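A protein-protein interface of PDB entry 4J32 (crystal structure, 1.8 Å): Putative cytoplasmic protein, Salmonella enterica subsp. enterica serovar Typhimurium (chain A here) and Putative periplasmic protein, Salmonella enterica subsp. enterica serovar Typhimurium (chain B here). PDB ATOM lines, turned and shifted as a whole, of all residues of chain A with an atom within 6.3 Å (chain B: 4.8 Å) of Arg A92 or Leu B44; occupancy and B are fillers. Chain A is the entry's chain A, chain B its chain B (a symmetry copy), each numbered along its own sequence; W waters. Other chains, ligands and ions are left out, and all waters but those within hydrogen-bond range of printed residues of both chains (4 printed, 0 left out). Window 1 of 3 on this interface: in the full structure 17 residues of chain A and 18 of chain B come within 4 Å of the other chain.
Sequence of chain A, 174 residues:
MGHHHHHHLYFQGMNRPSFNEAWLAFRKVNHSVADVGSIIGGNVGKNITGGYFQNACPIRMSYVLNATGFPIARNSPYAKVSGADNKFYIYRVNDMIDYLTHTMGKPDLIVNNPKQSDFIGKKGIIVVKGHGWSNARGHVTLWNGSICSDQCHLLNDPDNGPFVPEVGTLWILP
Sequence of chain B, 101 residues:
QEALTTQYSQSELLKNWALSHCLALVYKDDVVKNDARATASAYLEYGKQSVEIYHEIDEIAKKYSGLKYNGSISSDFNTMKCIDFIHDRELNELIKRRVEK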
ATOM      1  N   TYR A  52     -13.508   0.289  29.413  1.00  0.00           N
ATOM      2  CA  TYR A  52     -12.526  -0.302  28.491  1.00  0.00           C
ATOM      3  C   TYR A  52     -11.162   0.338  28.631  1.00  0.00           C
ATOM      4  O   TYR A  52     -10.151  -0.328  28.410  1.00  0.00           O
ATOM      5  CB  TYR A  52     -12.960  -0.142  27.032  1.00  0.00           C
ATOM      6  CG  TYR A  52     -14.262  -0.826  26.719  1.00  0.00           C
ATOM      7  CD1 TYR A  52     -14.277  -2.126  26.235  1.00  0.00           C
ATOM      8  CD2 TYR A  52     -15.481  -0.158  26.895  1.00  0.00           C
ATOM      9  CE1 TYR A  52     -15.487  -2.773  25.952  1.00  0.00           C
ATOM     10  CE2 TYR A  52     -16.696  -0.793  26.613  1.00  0.00           C
ATOM     11  CZ  TYR A  52     -16.676  -2.104  26.138  1.00  0.00           C
ATOM     12  OH  TYR A  52     -17.864  -2.731  25.837  1.00  0.00           O
ATOM     13  N   PHE A  53     -11.126   1.639  28.928  1.00  0.00           N
ATOM     14  CA  PHE A  53      -9.837   2.314  29.135  1.00  0.00           C
ATOM     15  C   PHE A  53      -9.736   2.643  30.606  1.00  0.00           C
ATOM     16  O   PHE A  53     -10.677   3.211  31.169  1.00  0.00           O
ATOM     17  CB  PHE A  53      -9.757   3.635  28.366  1.00  0.00           C
ATOM     18  CG  PHE A  53      -9.943   3.506  26.869  1.00  0.00           C
ATOM     19  CD1 PHE A  53      -9.691   2.303  26.204  1.00  0.00           C
ATOM     20  CD2 PHE A  53     -10.306   4.640  26.126  1.00  0.00           C
ATOM     21  CE1 PHE A  53      -9.836   2.201  24.813  1.00  0.00           C
ATOM     22  CE2 PHE A  53     -10.457   4.553  24.734  1.00  0.00           C
ATOM     23  CZ  PHE A  53     -10.234   3.333  24.084  1.00  0.00           C
ATOM     24  N   PRO A  58      -1.699   7.503  27.904  1.00  0.00           N
ATOM     25  CA  PRO A  58      -1.613   7.930  26.506  1.00  0.00           C
ATOM     26  C   PRO A  58      -2.707   8.906  26.075  1.00  0.00           C
ATOM     27  O   PRO A  58      -2.513   9.685  25.130  1.00  0.00           O
ATOM     28  CB  PRO A  58      -1.712   6.609  25.719  1.00  0.00           C
ATOM     29  CG  PRO A  58      -2.470   5.688  26.619  1.00  0.00           C
ATOM     30  CD  PRO A  58      -2.028   6.066  28.024  1.00  0.00           C
ATOM     31  N   ALA A  79      -3.889   2.670  17.069  1.00  0.00           N
ATOM     32  CA  ALA A  79      -5.270   2.610  17.519  1.00  0.00           C
ATOM     33  C   ALA A  79      -5.642   3.914  18.242  1.00  0.00           C
ATOM     34  O   ALA A  79      -4.892   4.403  19.087  1.00  0.00           O
ATOM     35  CB  ALA A  79      -5.485   1.384  18.427  1.00  0.00           C
ATOM     36  N   ILE A  90      -4.918   8.424  21.155  1.00  0.00           N
ATOM     37  CA  ILE A  90      -4.259   7.125  21.250  1.00  0.00           C
ATOM     38  C   ILE A  90      -4.429   6.571  22.664  1.00  0.00           C
ATOM     39  O   ILE A  90      -4.284   7.306  23.642  1.00  0.00           O
ATOM     40  CB  ILE A  90      -2.762   7.268  20.841  1.00  0.00           C
ATOM     41  CG1 ILE A  90      -2.657   7.476  19.314  1.00  0.00           C
ATOM     42  CG2 ILE A  90      -1.897   6.060  21.355  1.00  0.00           C
ATOM     43  CD1 ILE A  90      -1.204   7.854  18.837  1.00  0.00           C
ATOM     44  N   TYR A  91      -4.742   5.283  22.775  1.00  0.00           N
ATOM     45  CA  TYR A  91      -5.114   4.721  24.077  1.00  0.00           C
ATOM     46  C   TYR A  91      -4.171   3.635  24.603  1.00  0.00           C
ATOM     47  O   TYR A  91      -4.377   3.104  25.706  1.00  0.00           O
ATOM     48  CB  TYR A  91      -6.585   4.277  24.089  1.00  0.00           C
ATOM     49  CG  TYR A  91      -6.975   3.254  23.022  1.00  0.00           C
ATOM     50  CD1 TYR A  91      -6.776   1.898  23.236  1.00  0.00           C
ATOM     51  CD2 TYR A  91      -7.551   3.655  21.808  1.00  0.00           C
ATOM     52  CE1 TYR A  91      -7.152   0.940  22.279  1.00  0.00           C
ATOM     53  CE2 TYR A  91      -7.942   2.709  20.850  1.00  0.00           C
ATOM     54  CZ  TYR A  91      -7.757   1.353  21.104  1.00  0.00           C
ATOM     55  OH  TYR A  91      -8.098   0.395  20.178  1.00  0.00           O
ATOM     56  N   ARG A  92      -3.154   3.300  23.814  1.00  0.00           N
ATOM     57  CA  ARG A  92      -2.099   2.372  24.241  1.00  0.00           C
ATOM     58  C   ARG A  92      -0.781   3.110  24.473  1.00  0.00           C
ATOM     59  O   ARG A  92      -0.342   3.921  23.642  1.00  0.00           O
ATOM     60  CB  ARG A  92      -1.892   1.254  23.214  1.00  0.00           C
ATOM     61  CG  ARG A  92      -3.107   0.339  23.090  1.00  0.00           C
ATOM     62  CD  ARG A  92      -2.880  -0.784  22.048  1.00  0.00           C
ATOM     63  NE  ARG A  92      -3.913  -1.805  22.221  1.00  0.00           N
ATOM     64  CZ  ARG A  92      -4.814  -2.176  21.305  1.00  0.00           C
ATOM     65  NH1 ARG A  92      -4.797  -1.646  20.077  1.00  0.00           N
ATOM     66  NH2 ARG A  92      -5.717  -3.111  21.609  1.00  0.00           N
ATOM     67  N   VAL A  93      -0.147   2.795  25.597  1.00  0.00           N
ATOM     68  CA  VAL A  93       1.165   3.338  25.940  1.00  0.00           C
ATOM     69  C   VAL A  93       2.192   3.032  24.858  1.00  0.00           C
ATOM     70  O   VAL A  93       2.895   3.938  24.401  1.00  0.00           O
ATOM     71  CB  VAL A  93       1.658   2.810  27.307  1.00  0.00           C
ATOM     72  CG1 VAL A  93       3.113   3.318  27.574  1.00  0.00           C
ATOM     73  CG2 VAL A  93       0.695   3.321  28.409  1.00  0.00           C
ATOM     74  N   ASN A  94       2.253   1.780  24.413  1.00  0.00           N
ATOM     75  CA  ASN A  94       3.236   1.373  23.418  1.00  0.00           C
ATOM     76  C   ASN A  94       3.051   2.185  22.122  1.00  0.00           C
ATOM     77  O   ASN A  94       4.025   2.543  21.448  1.00  0.00           O
ATOM     78  CB  ASN A  94       3.149  -0.137  23.152  1.00  0.00           C
ATOM     79  CG  ASN A  94       3.989  -0.971  24.136  1.00  0.00           C
ATOM     80  OD1 ASN A  94       4.858  -0.439  24.849  1.00  0.00           O
ATOM     81  ND2 ASN A  94       3.764  -2.305  24.145  1.00  0.00           N
ATOM     82  N   ASP A  95       1.786   2.442  21.774  1.00  0.00           N
ATOM     83  CA  ASP A  95       1.456   3.206  20.565  1.00  0.00           C
ATOM     84  C   ASP A  95       1.866   4.662  20.708  1.00  0.00           C
ATOM     85  O   ASP A  95       2.422   5.241  19.779  1.00  0.00           O
ATOM     86  CB  ASP A  95      -0.044   3.128  20.221  1.00  0.00           C
ATOM     87  CG  ASP A  95      -0.415   1.838  19.511  1.00  0.00           C
ATOM     88  OD1 ASP A  95       0.497   1.042  19.138  1.00  0.00           O
ATOM     89  OD2 ASP A  95      -1.627   1.617  19.311  1.00  0.00           O
ATOM     90  N   MET A  96       1.644   5.237  21.880  1.00  0.00           N
ATOM     91  CA  MET A  96       2.010   6.635  22.103  1.00  0.00           C
ATOM     92  C   MET A  96       3.514   6.792  22.017  1.00  0.00           C
ATOM     93  O   MET A  96       4.018   7.745  21.393  1.00  0.00           O
ATOM     94  CB  MET A  96       1.503   7.157  23.453  1.00  0.00           C
ATOM     95  CG  MET A  96       2.002   8.591  23.779  1.00  0.00           C
ATOM     96  SD  MET A  96       1.674   9.853  22.509  1.00  0.00           S
ATOM     97  CE  MET A  96      -0.117   9.912  22.437  1.00  0.00           C
ATOM     98  N   ILE A  97       4.237   5.847  22.615  1.00  0.00           N
ATOM     99  CA  ILE A  97       5.703   5.851  22.532  1.00  0.00           C
ATOM    100  C   ILE A  97       6.167   5.804  21.071  1.00  0.00           C
ATOM    101  O   ILE A  97       7.015   6.621  20.650  1.00  0.00           O
ATOM    102  CB  ILE A  97       6.319   4.696  23.363  1.00  0.00           C
ATOM    103  CG1 ILE A  97       6.059   4.964  24.848  1.00  0.00           C
ATOM    104  CG2 ILE A  97       7.849   4.624  23.115  1.00  0.00           C
ATOM    105  CD1 ILE A  97       6.445   3.799  25.793  1.00  0.00           C
ATOM    106  N   TRP B  17      -8.727 -10.997  28.284  1.00  0.00           N
ATOM    107  CA  TRP B  17      -9.606  -9.837  28.312  1.00  0.00           C
ATOM    108  C   TRP B  17     -11.057 -10.257  28.500  1.00  0.00           C
ATOM    109  O   TRP B  17     -11.765  -9.699  29.331  1.00  0.00           O
ATOM    110  CB  TRP B  17      -9.453  -8.965  27.038  1.00  0.00           C
ATOM    111  CG  TRP B  17     -10.087  -7.603  27.231  1.00  0.00           C
ATOM    112  CD1 TRP B  17      -9.456  -6.476  27.652  1.00  0.00           C
ATOM    113  CD2 TRP B  17     -11.466  -7.254  27.059  1.00  0.00           C
ATOM    114  NE1 TRP B  17     -10.344  -5.440  27.751  1.00  0.00           N
ATOM    115  CE2 TRP B  17     -11.590  -5.886  27.397  1.00  0.00           C
ATOM    116  CE3 TRP B  17     -12.608  -7.961  26.634  1.00  0.00           C
ATOM    117  CZ2 TRP B  17     -12.818  -5.192  27.329  1.00  0.00           C
ATOM    118  CZ3 TRP B  17     -13.827  -7.281  26.573  1.00  0.00           C
ATOM    119  CH2 TRP B  17     -13.926  -5.903  26.909  1.00  0.00           C
ATOM    120  N   ALA B  40      -8.352  -6.310  32.980  1.00  0.00           N
ATOM    121  CA  ALA B  40      -8.701  -6.329  31.556  1.00  0.00           C
ATOM    122  C   ALA B  40      -7.905  -5.264  30.777  1.00  0.00           C
ATOM    123  O   ALA B  40      -7.424  -5.535  29.678  1.00  0.00           O
ATOM    124  CB  ALA B  40     -10.218  -6.148  31.348  1.00  0.00           C
ATOM    125  N   SER B  41      -7.714  -4.084  31.367  1.00  0.00           N
ATOM    126  CA  SER B  41      -7.045  -2.996  30.633  1.00  0.00           C
ATOM    127  C   SER B  41      -5.581  -3.397  30.297  1.00  0.00           C
ATOM    128  O   SER B  41      -5.032  -2.968  29.272  1.00  0.00           O
ATOM    129  CB  SER B  41      -7.113  -1.664  31.390  1.00  0.00           C
ATOM    130  OG  SER B  41      -6.209  -1.618  32.469  1.00  0.00           O
ATOM    131  N   ALA B  42      -4.977  -4.224  31.145  1.00  0.00           N
ATOM    132  CA  ALA B  42      -3.608  -4.706  30.906  1.00  0.00           C
ATOM    133  C   ALA B  42      -3.570  -5.554  29.628  1.00  0.00           C
ATOM    134  O   ALA B  42      -2.653  -5.424  28.798  1.00  0.00           O
ATOM    135  CB  ALA B  42      -3.101  -5.513  32.106  1.00  0.00           C
ATOM    136  N   TYR B  43      -4.568  -6.424  29.453  1.00  0.00           N
ATOM    137  CA  TYR B  43      -4.607  -7.250  28.225  1.00  0.00           C
ATOM    138  C   TYR B  43      -4.909  -6.416  26.976  1.00  0.00           C
ATOM    139  O   TYR B  43      -4.375  -6.710  25.896  1.00  0.00           O
ATOM    140  CB  TYR B  43      -5.593  -8.414  28.370  1.00  0.00           C
ATOM    141  CG  TYR B  43      -5.218  -9.267  29.555  1.00  0.00           C
ATOM    142  CD1 TYR B  43      -3.924  -9.797  29.658  1.00  0.00           C
ATOM    143  CD2 TYR B  43      -6.130  -9.496  30.596  1.00  0.00           C
ATOM    144  CE1 TYR B  43      -3.523 -10.562  30.767  1.00  0.00           C
ATOM    145  CE2 TYR B  43      -5.752 -10.275  31.714  1.00  0.00           C
ATOM    146  CZ  TYR B  43      -4.458 -10.801  31.781  1.00  0.00           C
ATOM    147  OH  TYR B  43      -4.054 -11.529  32.860  1.00  0.00           O
ATOM    148  N   LEU B  44      -5.767  -5.404  27.116  1.00  0.00           N
ATOM    149  CA  LEU B  44      -6.014  -4.459  26.012  1.00  0.00           C
ATOM    150  C   LEU B  44      -4.744  -3.714  25.585  1.00  0.00           C
ATOM    151  O   LEU B  44      -4.535  -3.506  24.381  1.00  0.00           O
ATOM    152  CB  LEU B  44      -7.176  -3.487  26.340  1.00  0.00           C
ATOM    153  CG  LEU B  44      -7.577  -2.446  25.279  1.00  0.00           C
ATOM    154  CD1 LEU B  44      -9.076  -2.177  25.390  1.00  0.00           C
ATOM    155  CD2 LEU B  44      -6.768  -1.191  25.437  1.00  0.00           C
ATOM    156  N   GLU B  45      -3.906  -3.313  26.548  1.00  0.00           N
ATOM    157  CA  GLU B  45      -2.674  -2.573  26.246  1.00  0.00           C
ATOM    158  C   GLU B  45      -1.818  -3.323  25.232  1.00  0.00           C
ATOM    159  O   GLU B  45      -1.240  -2.705  24.319  1.00  0.00           O
ATOM    160  CB  GLU B  45      -1.845  -2.292  27.514  1.00  0.00           C
ATOM    161  CG  GLU B  45      -0.355  -1.881  27.300  1.00  0.00           C
ATOM    162  CD  GLU B  45      -0.153  -0.489  26.662  1.00  0.00           C
ATOM    163  OE1 GLU B  45      -1.033   0.397  26.853  1.00  0.00           O
ATOM    164  OE2 GLU B  45       0.889  -0.280  25.987  1.00  0.00           O
ATOM    165  N   TYR B  46      -1.706  -4.637  25.414  1.00  0.00           N
ATOM    166  CA  TYR B  46      -0.792  -5.459  24.594  1.00  0.00           C
ATOM    167  C   TYR B  46      -1.422  -6.007  23.311  1.00  0.00           C
ATOM    168  O   TYR B  46      -0.725  -6.591  22.452  1.00  0.00           O
ATOM    169  CB  TYR B  46      -0.212  -6.585  25.446  1.00  0.00           C
ATOM    170  CG  TYR B  46       0.775  -6.091  26.491  1.00  0.00           C
ATOM    171  CD1 TYR B  46       2.079  -5.732  26.135  1.00  0.00           C
ATOM    172  CD2 TYR B  46       0.398  -5.949  27.821  1.00  0.00           C
ATOM    173  CE1 TYR B  46       3.008  -5.272  27.108  1.00  0.00           C
ATOM    174  CE2 TYR B  46       1.317  -5.476  28.797  1.00  0.00           C
ATOM    175  CZ  TYR B  46       2.610  -5.151  28.428  1.00  0.00           C
ATOM    176  OH  TYR B  46       3.530  -4.722  29.391  1.00  0.00           O
ATOM    177  N   GLY B  47      -2.725  -5.806  23.163  1.00  0.00           N
ATOM    178  CA  GLY B  47      -3.416  -6.207  21.919  1.00  0.00           C
ATOM    179  C   GLY B  47      -3.041  -5.338  20.726  1.00  0.00           C
ATOM    180  O   GLY B  47      -2.565  -4.216  20.887  1.00  0.00           O
ATOM    181  N   LYS B  48      -3.222  -5.882  19.521  1.00  0.00           N
ATOM    182  CA  LYS B  48      -2.973  -5.154  18.277  1.00  0.00           C
ATOM    183  C   LYS B  48      -4.302  -4.891  17.552  1.00  0.00           C
ATOM    184  O   LYS B  48      -4.315  -4.424  16.398  1.00  0.00           O
ATOM    185  CB  LYS B  48      -2.014  -5.951  17.363  1.00  0.00           C
ATOM    186  CG  LYS B  48      -0.594  -6.190  17.956  1.00  0.00           C
ATOM    187  CD  LYS B  48       0.045  -4.865  18.374  1.00  0.00           C
ATOM    188  CE  LYS B  48       1.526  -4.996  18.724  1.00  0.00           C
ATOM    189  NZ  LYS B  48       2.201  -3.646  18.633  1.00  0.00           N
ATOM    190  N   GLN B  49      -5.398  -5.145  18.265  1.00  0.00           N
ATOM    191  CA  GLN B  49      -6.749  -5.034  17.697  1.00  0.00           C
ATOM    192  C   GLN B  49      -7.376  -3.693  18.016  1.00  0.00           C
ATOM    193  O   GLN B  49      -7.075  -3.070  19.055  1.00  0.00           O
ATOM    194  CB  GLN B  49      -7.683  -6.149  18.216  1.00  0.00           C
ATOM    195  CG  GLN B  49      -7.261  -7.581  17.804  1.00  0.00           C
ATOM    196  CD  GLN B  49      -5.996  -8.043  18.533  1.00  0.00           C
ATOM    197  OE1 GLN B  49      -5.856  -7.846  19.739  1.00  0.00           O
ATOM    198  NE2 GLN B  49      -5.069  -8.659  17.798  1.00  0.00           N
ATOM    199  N   TYR B  54     -13.183  -5.558  21.293  1.00  0.00           N
ATOM    200  CA  TYR B  54     -13.517  -5.646  22.716  1.00  0.00           C
ATOM    201  C   TYR B  54     -14.997  -5.316  22.974  1.00  0.00           C
ATOM    202  O   TYR B  54     -15.629  -5.941  23.839  1.00  0.00           O
ATOM    203  CB  TYR B  54     -12.597  -4.724  23.531  1.00  0.00           C
ATOM    204  CG  TYR B  54     -11.139  -4.981  23.255  1.00  0.00           C
ATOM    205  CD1 TYR B  54     -10.428  -5.931  24.002  1.00  0.00           C
ATOM    206  CD2 TYR B  54     -10.463  -4.261  22.257  1.00  0.00           C
ATOM    207  CE1 TYR B  54      -9.071  -6.174  23.767  1.00  0.00           C
ATOM    208  CE2 TYR B  54      -9.093  -4.503  21.998  1.00  0.00           C
ATOM    209  CZ  TYR B  54      -8.416  -5.441  22.760  1.00  0.00           C
ATOM    210  OH  TYR B  54      -7.084  -5.682  22.527  1.00  0.00           O
HETATM  211  O   HOH W   1       3.353  -0.852  27.135  1.00  0.00           O
HETATM  212  O   HOH W   2      -9.948  -2.991  29.012  1.00  0.00           O
HETATM  213  O   HOH W   3       0.602  -1.552  19.848  1.00  0.00           O
HETATM  214  O   HOH W   4      -3.761   0.562  26.791  1.00  0.00           O
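Water W3 bridges OD1 of Asp A95 (2.7 Å) and NZ of Lys B48 (2.9 Å). Water W4 bridges the side-chain carboxylate (OE1) of Glu B45 and the backbone carbonyl oxygen (O) of Tyr A91. Water W2 lies within hydrogen-bond range of the backbone carbonyl oxygen of Tyr A52 (2.7 Å), the indole nitrogen of Trp B17 (2.8 Å) and the backbone NH of Ser B41 (3.4 Å). Water W1 bridges OD1 of Asn A94 and OE2 of Glu B45.
Of the 12 printed residues of chain A, 5 touch a printed residue of chain B. Hydrophobic or aromatic side chains of chain A within 4 Å of the printed part of chain B: Tyr A52, Tyr A91 and Val A93. Of the 12 printed residues of chain B, 6 touch a printed residue of chain A. Among the printed residues, no Asp or Glu carboxylate lies within 4 Å of a Lys or Arg side-chain nitrogen of the other chain.
NE1 of Trp B17 sits close to O of Ala B40 (3.5 Å).
O of Gln B49 lies within hydrogen-bond range of NH1 of Arg A92. The backbone carbonyl oxygen (O) of Leu B44 is in hydrogen-bond range of the guanidinium group (NE) of Arg A92 (2.8 Å). The backbone carbonyl oxygen of Gly B47 lies close to the guanidinium group of Arg A92 (3.1 Å). The backbone NH (N) of Val A93 lies within hydrogen-bond range of the side-chain carboxylate (OE1) of Glu B45, at 2.8 Å. The guanidinium group (NH2) of Arg A92 sits at hydrogen-bond distance from the side-chain hydroxyl (OH) of Tyr B54, 3.1 Å away. OE2 of Glu B45 lies within hydrogen-bond range of N of Asn A94, 2.9 Å away.
Tyr A52 touches Trp B17 (CD1 to CZ2, 3.6 Å). CD1 of Leu B44 touches O of Tyr A52, at 3.7 Å. Tyr A52 touches Tyr B54 (CE1 to O, 3.8 Å). Leu B44 touches Tyr A91 (CD2 to CD1, 3.8 Å). Gln B49 touches Tyr A91 (O to OH, 3.8 Å). Arg A92 touches Glu B45 (CD to O, 3.4 Å).
Of the printed residues of chain B, Tyr A52 touches Trp B17 (3.6 Å), Leu B44 (3.7 Å) and Tyr B54 (3.8 Å). Printed residues of chain B within 4 Å of Arg A92: Leu B44, Glu B45, Gly B47, Gln B49 and Tyr B54. Printed residues of chain B within 4 Å of Val A93: Glu B45 (2.8 Å). Ile A97 touches none of the printed residues of chain B. Ala B42 touches none of the printed residues of chain A. Of chain A, only Tyr A52, Tyr A91 and Arg A92 come within 4 Å of Leu B44. Of the printed residues of chain A, Glu B45 touches Arg A92 (3.4 Å), Val A93 (2.8 Å) and Asn A94 (2.9 Å). Printed residues of chain A within 4 Å of Gln B49: Tyr A91 and Arg A92. Of the printed residues of chain A, Tyr B54 touches Tyr A52 (3.8 Å) and Arg A92 (3.1 Å). The nearest residue of chain A that does not touch Leu B44 is Phe A53 (4.5 Å).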
